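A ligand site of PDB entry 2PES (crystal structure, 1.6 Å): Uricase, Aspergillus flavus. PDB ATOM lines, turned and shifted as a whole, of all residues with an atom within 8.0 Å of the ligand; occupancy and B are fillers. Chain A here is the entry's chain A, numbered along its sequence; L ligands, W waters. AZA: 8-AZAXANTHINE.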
ATOM      1  N   SER A 157      35.540 -22.332  11.809  1.00  0.00           N
ATOM      2  CA  SER A 157      34.201 -22.664  11.360  1.00  0.00           C
ATOM      3  C   SER A 157      34.110 -22.217   9.902  1.00  0.00           C
ATOM      4  O   SER A 157      34.554 -21.134   9.546  1.00  0.00           O
ATOM      5  CB  SER A 157      33.146 -21.975  12.222  1.00  0.00           C
ATOM      6  OG  SER A 157      31.840 -22.167  11.680  1.00  0.00           O
ATOM      7  N   GLN A 158      33.583 -23.093   9.053  1.00  0.00           N
ATOM      8  CA  GLN A 158      33.405 -22.816   7.635  1.00  0.00           C
ATOM      9  C   GLN A 158      31.983 -23.120   7.237  1.00  0.00           C
ATOM     10  O   GLN A 158      31.272 -23.848   7.910  1.00  0.00           O
ATOM     11  CB  GLN A 158      34.324 -23.721   6.801  1.00  0.00           C
ATOM     12  CG  GLN A 158      35.804 -23.569   7.172  1.00  0.00           C
ATOM     13  CD  GLN A 158      36.699 -24.539   6.434  1.00  0.00           C
ATOM     14  OE1 GLN A 158      36.351 -25.065   5.387  1.00  0.00           O
ATOM     15  NE2 GLN A 158      37.857 -24.789   7.017  1.00  0.00           N
ATOM     16  N   PHE A 159      31.555 -22.534   6.130  1.00  0.00           N
ATOM     17  CA  PHE A 159      30.276 -22.921   5.525  1.00  0.00           C
ATOM     18  C   PHE A 159      30.283 -22.621   4.024  1.00  0.00           C
ATOM     19  O   PHE A 159      30.129 -21.482   3.591  1.00  0.00           O
ATOM     20  CB  PHE A 159      29.063 -22.291   6.235  1.00  0.00           C
ATOM     21  CG  PHE A 159      27.732 -22.893   5.784  1.00  0.00           C
ATOM     22  CD1 PHE A 159      27.493 -24.255   6.008  1.00  0.00           C
ATOM     23  CD2 PHE A 159      26.768 -22.159   5.103  1.00  0.00           C
ATOM     24  CE1 PHE A 159      26.329 -24.842   5.590  1.00  0.00           C
ATOM     25  CE2 PHE A 159      25.586 -22.763   4.683  1.00  0.00           C
ATOM     26  CZ  PHE A 159      25.369 -24.107   4.932  1.00  0.00           C
ATOM     27  N   TRP A 160      30.553 -23.669   3.252  1.00  0.00           N
ATOM     28  CA  TRP A 160      30.570 -23.572   1.802  1.00  0.00           C
ATOM     29  C   TRP A 160      30.025 -24.864   1.192  1.00  0.00           C
ATOM     30  O   TRP A 160      29.805 -25.853   1.896  1.00  0.00           O
ATOM     31  CB  TRP A 160      31.991 -23.290   1.283  1.00  0.00           C
ATOM     32  CG  TRP A 160      33.027 -24.239   1.804  1.00  0.00           C
ATOM     33  CD1 TRP A 160      33.823 -24.049   2.876  1.00  0.00           C
ATOM     34  CD2 TRP A 160      33.401 -25.518   1.250  1.00  0.00           C
ATOM     35  NE1 TRP A 160      34.654 -25.115   3.062  1.00  0.00           N
ATOM     36  CE2 TRP A 160      34.412 -26.034   2.078  1.00  0.00           C
ATOM     37  CE3 TRP A 160      32.966 -26.272   0.170  1.00  0.00           C
ATOM     38  CZ2 TRP A 160      35.003 -27.276   1.853  1.00  0.00           C
ATOM     39  CZ3 TRP A 160      33.572 -27.531  -0.053  1.00  0.00           C
ATOM     40  CH2 TRP A 160      34.565 -27.985   0.774  1.00  0.00           C
ATOM     41  N   PHE A 162      27.040 -25.268  -0.172  1.00  0.00           N
ATOM     42  CA  PHE A 162      25.588 -25.374  -0.069  1.00  0.00           C
ATOM     43  C   PHE A 162      24.919 -25.102  -1.410  1.00  0.00           C
ATOM     44  O   PHE A 162      25.564 -24.593  -2.352  1.00  0.00           O
ATOM     45  CB  PHE A 162      25.035 -24.451   1.030  1.00  0.00           C
ATOM     46  CG  PHE A 162      25.512 -23.036   0.913  1.00  0.00           C
ATOM     47  CD1 PHE A 162      26.662 -22.644   1.576  1.00  0.00           C
ATOM     48  CD2 PHE A 162      24.810 -22.117   0.159  1.00  0.00           C
ATOM     49  CE1 PHE A 162      27.138 -21.332   1.464  1.00  0.00           C
ATOM     50  CE2 PHE A 162      25.272 -20.820   0.037  1.00  0.00           C
ATOM     51  CZ  PHE A 162      26.435 -20.428   0.694  1.00  0.00           C
ATOM     52  N   LEU A 170      23.689 -15.782   0.037  1.00  0.00           N
ATOM     53  CA  LEU A 170      24.761 -16.034   0.997  1.00  0.00           C
ATOM     54  C   LEU A 170      26.086 -16.372   0.337  1.00  0.00           C
ATOM     55  O   LEU A 170      26.133 -17.246  -0.531  1.00  0.00           O
ATOM     56  CB  LEU A 170      24.369 -17.214   1.912  1.00  0.00           C
ATOM     57  CG  LEU A 170      25.331 -17.569   3.044  1.00  0.00           C
ATOM     58  CD1 LEU A 170      25.365 -16.461   4.078  1.00  0.00           C
ATOM     59  CD2 LEU A 170      24.932 -18.867   3.677  1.00  0.00           C
ATOM     60  N   LYS A 171      27.137 -15.671   0.726  1.00  0.00           N
ATOM     61  CA  LYS A 171      28.482 -15.963   0.244  1.00  0.00           C
ATOM     62  C   LYS A 171      29.079 -17.166   0.976  1.00  0.00           C
ATOM     63  O   LYS A 171      28.990 -17.308   2.202  1.00  0.00           O
ATOM     64  CB  LYS A 171      29.382 -14.739   0.393  1.00  0.00           C
ATOM     65  CG  LYS A 171      28.992 -13.580  -0.553  1.00  0.00           C
ATOM     66  CD  LYS A 171      29.898 -12.369  -0.403  1.00  0.00           C
ATOM     67  CE  LYS A 171      29.612 -11.338  -1.496  1.00  0.00           C
ATOM     68  NZ  LYS A 171      30.231  -9.990  -1.222  1.00  0.00           N
ATOM     69  N   THR A 173      31.959 -19.196   2.793  1.00  0.00           N
ATOM     70  CA  THR A 173      33.018 -18.743   3.680  1.00  0.00           C
ATOM     71  C   THR A 173      33.887 -19.889   4.175  1.00  0.00           C
ATOM     72  O   THR A 173      33.386 -20.978   4.449  1.00  0.00           O
ATOM     73  CB  THR A 173      32.477 -17.939   4.899  1.00  0.00           C
ATOM     74  OG1 THR A 173      33.586 -17.446   5.649  1.00  0.00           O
ATOM     75  CG2 THR A 173      31.607 -18.797   5.793  1.00  0.00           C
ATOM     76  N   ARG A 176      34.493 -18.220   9.588  1.00  0.00           N
ATOM     77  CA  ARG A 176      33.456 -17.421  10.219  1.00  0.00           C
ATOM     78  C   ARG A 176      33.447 -17.675  11.719  1.00  0.00           C
ATOM     79  O   ARG A 176      34.043 -18.607  12.221  1.00  0.00           O
ATOM     80  CB  ARG A 176      32.075 -17.767   9.670  1.00  0.00           C
ATOM     81  CG  ARG A 176      31.664 -19.198   9.946  1.00  0.00           C
ATOM     82  CD  ARG A 176      30.296 -19.522   9.387  1.00  0.00           C
ATOM     83  NE  ARG A 176      29.874 -20.837   9.858  1.00  0.00           N
ATOM     84  CZ  ARG A 176      28.667 -21.357   9.664  1.00  0.00           C
ATOM     85  NH1 ARG A 176      27.746 -20.712   8.977  1.00  0.00           N
ATOM     86  NH2 ARG A 176      28.408 -22.555  10.137  1.00  0.00           N
ATOM     87  N   LEU A 178      31.334 -18.870  14.915  1.00  0.00           N
ATOM     88  CA  LEU A 178      30.223 -19.776  15.219  1.00  0.00           C
ATOM     89  C   LEU A 178      29.845 -19.623  16.681  1.00  0.00           C
ATOM     90  O   LEU A 178      30.658 -19.767  17.569  1.00  0.00           O
ATOM     91  CB  LEU A 178      30.591 -21.229  14.908  1.00  0.00           C
ATOM     92  CG  LEU A 178      29.518 -22.270  15.159  1.00  0.00           C
ATOM     93  CD1 LEU A 178      28.262 -21.940  14.420  1.00  0.00           C
ATOM     94  CD2 LEU A 178      30.043 -23.661  14.797  1.00  0.00           C
ATOM     95  N   SER A 224      34.835 -27.026  11.872  1.00  0.00           N
ATOM     96  CA  SER A 224      33.433 -27.287  11.573  1.00  0.00           C
ATOM     97  C   SER A 224      33.060 -26.968  10.114  1.00  0.00           C
ATOM     98  O   SER A 224      33.302 -25.871   9.629  1.00  0.00           O
ATOM     99  CB  SER A 224      32.573 -26.454  12.514  1.00  0.00           C
ATOM    100  OG  SER A 224      31.223 -26.539  12.184  1.00  0.00           O
ATOM    101  N   ALA A 225      32.446 -27.942   9.437  1.00  0.00           N
ATOM    102  CA  ALA A 225      31.953 -27.788   8.062  1.00  0.00           C
ATOM    103  C   ALA A 225      30.541 -27.198   8.022  1.00  0.00           C
ATOM    104  O   ALA A 225      30.092 -26.699   7.007  1.00  0.00           O
ATOM    105  CB  ALA A 225      31.960 -29.141   7.384  1.00  0.00           C
ATOM    106  N   SER A 226      29.858 -27.258   9.158  1.00  0.00           N
ATOM    107  CA  SER A 226      28.516 -26.797   9.328  1.00  0.00           C
ATOM    108  C   SER A 226      28.122 -27.098  10.761  1.00  0.00           C
ATOM    109  O   SER A 226      28.735 -27.936  11.408  1.00  0.00           O
ATOM    110  CB  SER A 226      27.519 -27.485   8.393  1.00  0.00           C
ATOM    111  OG  SER A 226      27.372 -28.862   8.698  1.00  0.00           O
ATOM    112  N   VAL A 227      27.042 -26.481  11.210  1.00  0.00           N
ATOM    113  CA  VAL A 227      26.470 -26.820  12.510  1.00  0.00           C
ATOM    114  C   VAL A 227      26.001 -28.278  12.507  1.00  0.00           C
ATOM    115  O   VAL A 227      26.258 -29.007  13.456  1.00  0.00           O
ATOM    116  CB  VAL A 227      25.304 -25.877  12.853  1.00  0.00           C
ATOM    117  CG1 VAL A 227      24.609 -26.329  14.137  1.00  0.00           C
ATOM    118  CG2 VAL A 227      25.842 -24.449  12.991  1.00  0.00           C
ATOM    119  N   GLN A 228      25.343 -28.660  11.420  1.00  0.00           N
ATOM    120  CA  GLN A 228      24.878 -30.040  11.193  1.00  0.00           C
ATOM    121  C   GLN A 228      25.992 -31.046  11.462  1.00  0.00           C
ATOM    122  O   GLN A 228      25.828 -32.027  12.215  1.00  0.00           O
ATOM    123  CB  GLN A 228      24.379 -30.198   9.764  1.00  0.00           C
ATOM    124  CG  GLN A 228      23.063 -29.516   9.477  1.00  0.00           C
ATOM    125  CD  GLN A 228      23.158 -28.061   9.047  1.00  0.00           C
ATOM    126  OE1 GLN A 228      24.119 -27.352   9.342  1.00  0.00           O
ATOM    127  NE2 GLN A 228      22.112 -27.594   8.369  1.00  0.00           N
ATOM    128  N   ALA A 229      27.148 -30.829  10.833  1.00  0.00           N
ATOM    129  CA  ALA A 229      28.229 -31.792  10.908  1.00  0.00           C
ATOM    130  C   ALA A 229      28.839 -31.869  12.310  1.00  0.00           C
ATOM    131  O   ALA A 229      29.144 -32.954  12.801  1.00  0.00           O
ATOM    132  CB  ALA A 229      29.284 -31.443   9.888  1.00  0.00           C
ATOM    133  N   THR A 230      28.967 -30.724  12.957  1.00  0.00           N
ATOM    134  CA  THR A 230      29.563 -30.678  14.285  1.00  0.00           C
ATOM    135  C   THR A 230      28.633 -31.329  15.322  1.00  0.00           C
ATOM    136  O   THR A 230      29.103 -32.061  16.205  1.00  0.00           O
ATOM    137  CB  THR A 230      29.926 -29.238  14.664  1.00  0.00           C
ATOM    138  OG1 THR A 230      30.908 -28.774  13.745  1.00  0.00           O
ATOM    139  CG2 THR A 230      30.488 -29.166  16.064  1.00  0.00           C
ATOM    140  N   ASN A 254      21.907 -20.968  15.344  1.00  0.00           N
ATOM    141  CA  ASN A 254      23.129 -20.402  14.770  1.00  0.00           C
ATOM    142  C   ASN A 254      22.954 -18.886  14.947  1.00  0.00           C
ATOM    143  O   ASN A 254      22.119 -18.264  14.280  1.00  0.00           O
ATOM    144  CB  ASN A 254      23.280 -20.803  13.289  1.00  0.00           C
ATOM    145  CG  ASN A 254      24.623 -20.437  12.703  1.00  0.00           C
ATOM    146  OD1 ASN A 254      25.502 -19.900  13.378  1.00  0.00           O
ATOM    147  ND2 ASN A 254      24.808 -20.748  11.418  1.00  0.00           N
ATOM    148  N   HIS A 256      24.026 -15.384  14.508  1.00  0.00           N
ATOM    149  CA  HIS A 256      24.896 -14.800  13.460  1.00  0.00           C
ATOM    150  C   HIS A 256      25.640 -13.561  13.939  1.00  0.00           C
ATOM    151  O   HIS A 256      25.087 -12.739  14.651  1.00  0.00           O
ATOM    152  CB  HIS A 256      24.058 -14.459  12.243  1.00  0.00           C
ATOM    153  CG  HIS A 256      23.260 -15.618  11.717  1.00  0.00           C
ATOM    154  ND1 HIS A 256      23.844 -16.797  11.315  1.00  0.00           N
ATOM    155  CD2 HIS A 256      21.925 -15.785  11.551  1.00  0.00           C
ATOM    156  CE1 HIS A 256      22.902 -17.648  10.911  1.00  0.00           C
ATOM    157  NE2 HIS A 256      21.730 -17.049  11.056  1.00  0.00           N
ATOM    158  N   GLY A 286      19.489 -19.084  12.485  1.00  0.00           N
ATOM    159  CA  GLY A 286      19.353 -20.463  12.008  1.00  0.00           C
ATOM    160  C   GLY A 286      18.946 -21.328  13.181  1.00  0.00           C
ATOM    161  O   GLY A 286      19.259 -21.014  14.335  1.00  0.00           O
ATOM    162  N   LEU A 287      18.242 -22.417  12.884  1.00  0.00           N
ATOM    163  CA  LEU A 287      17.867 -23.391  13.917  1.00  0.00           C
ATOM    164  C   LEU A 287      18.084 -24.774  13.323  1.00  0.00           C
ATOM    165  O   LEU A 287      17.512 -25.078  12.284  1.00  0.00           O
ATOM    166  CB  LEU A 287      16.431 -23.226  14.337  1.00  0.00           C
ATOM    167  CG  LEU A 287      15.920 -24.152  15.437  1.00  0.00           C
ATOM    168  CD1 LEU A 287      16.801 -24.081  16.683  1.00  0.00           C
ATOM    169  CD2 LEU A 287      14.474 -23.804  15.744  1.00  0.00           C
ATOM    170  N   ILE A 288      18.943 -25.548  13.959  1.00  0.00           N
ATOM    171  CA  ILE A 288      19.435 -26.817  13.403  1.00  0.00           C
ATOM    172  C   ILE A 288      19.172 -27.902  14.434  1.00  0.00           C
ATOM    173  O   ILE A 288      19.588 -27.774  15.582  1.00  0.00           O
ATOM    174  CB  ILE A 288      20.929 -26.749  13.083  1.00  0.00           C
ATOM    175  CG1 ILE A 288      21.341 -25.401  12.402  1.00  0.00           C
ATOM    176  CG2 ILE A 288      21.316 -27.957  12.262  1.00  0.00           C
ATOM    177  CD1 ILE A 288      20.705 -25.133  11.130  1.00  0.00           C
HETATM  178  N1  AZA L   1      24.255 -24.551   8.541  1.00  0.00           N
HETATM  179  C2  AZA L   1      25.275 -23.723   8.917  1.00  0.00           C
HETATM  180  O2  AZA L   1      26.150 -24.183   9.679  1.00  0.00           O
HETATM  181  N3  AZA L   1      25.344 -22.402   8.530  1.00  0.00           N
HETATM  182  C4  AZA L   1      24.379 -21.965   7.699  1.00  0.00           C
HETATM  183  C5  AZA L   1      23.329 -22.755   7.253  1.00  0.00           C
HETATM  184  C6  AZA L   1      23.280 -24.159   7.717  1.00  0.00           C
HETATM  185  O6  AZA L   1      22.345 -24.899   7.368  1.00  0.00           O
HETATM  186  N7  AZA L   1      22.547 -22.036   6.444  1.00  0.00           N
HETATM  187  N8  AZA L   1      23.118 -20.779   6.426  1.00  0.00           N
HETATM  188  N9  AZA L   1      24.268 -20.723   7.201  1.00  0.00           N
HETATM  189  O   HOH W   1      25.514 -18.336   7.872  1.00  0.00           O
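A nitrogen (N3) of the ligand sits close to the side-chain amide nitrogen (ND2) of Asn 254, at 3.4 Å. An oxygen (O2) of the ligand is in hydrogen-bond range of the guanidinium group of Arg 176, at 2.8 Å. The backbone NH (N) of Val 227 lies within hydrogen-bond range of an oxygen (O2) of the ligand (2.9 Å). An oxygen (O6) of the ligand is in hydrogen-bond range of the side-chain amide nitrogen of Gln 228, 2.9 Å away.
The backbone NH (N) of Asn 254 sits at hydrogen-bond distance from the backbone carbonyl oxygen (O) of Gly 286 (2.8 Å). The backbone NH (N) of Ala 229 sits at hydrogen-bond distance from the side-chain hydroxyl (OG) of Ser 226, at 2.9 Å. The backbone NH (N) of Arg 176 lies within hydrogen-bond range of the backbone carbonyl oxygen (O) of Ser 157. The backbone NH of Phe 159 sits at hydrogen-bond distance from the backbone carbonyl oxygen of Thr 173 (2.9 Å). O of Ser 226 sits at hydrogen-bond distance from OG of Ser 224 (3.0 Å). A ring nitrogen (NE2) of His 256 is in hydrogen-bond range of the backbone carbonyl oxygen (O) of Asn 254 (3.5 Å). The backbone NH (N) of Gln 228 sits close to the side-chain hydroxyl (OG) of Ser 226 (3.4 Å). The side-chain hydroxyl (OG1) of Thr 230 is in hydrogen-bond range of the backbone carbonyl oxygen (O) of Ser 226 (3.3 Å).
Water W1 bridges a nitrogen (N9) of the ligand (2.8 Å) and the guanidinium group (NH1) of Arg 176 (3.4 Å).
CE2 of Phe 159 touches C4 of the ligand, at 3.3 Å. Leu 170 touches the ligand (CD2 to N8, 3.8 Å). Ser 226 touches the ligand. Hydrophobic or aromatic side chains that line the ligand: Phe 159, Leu 170 and Val 227. Of the 22 residues printed, 7 come within 4 Å of the ligand. The nearest printed residue that does not touch the ligand is Ile 288 (4.1 Å).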
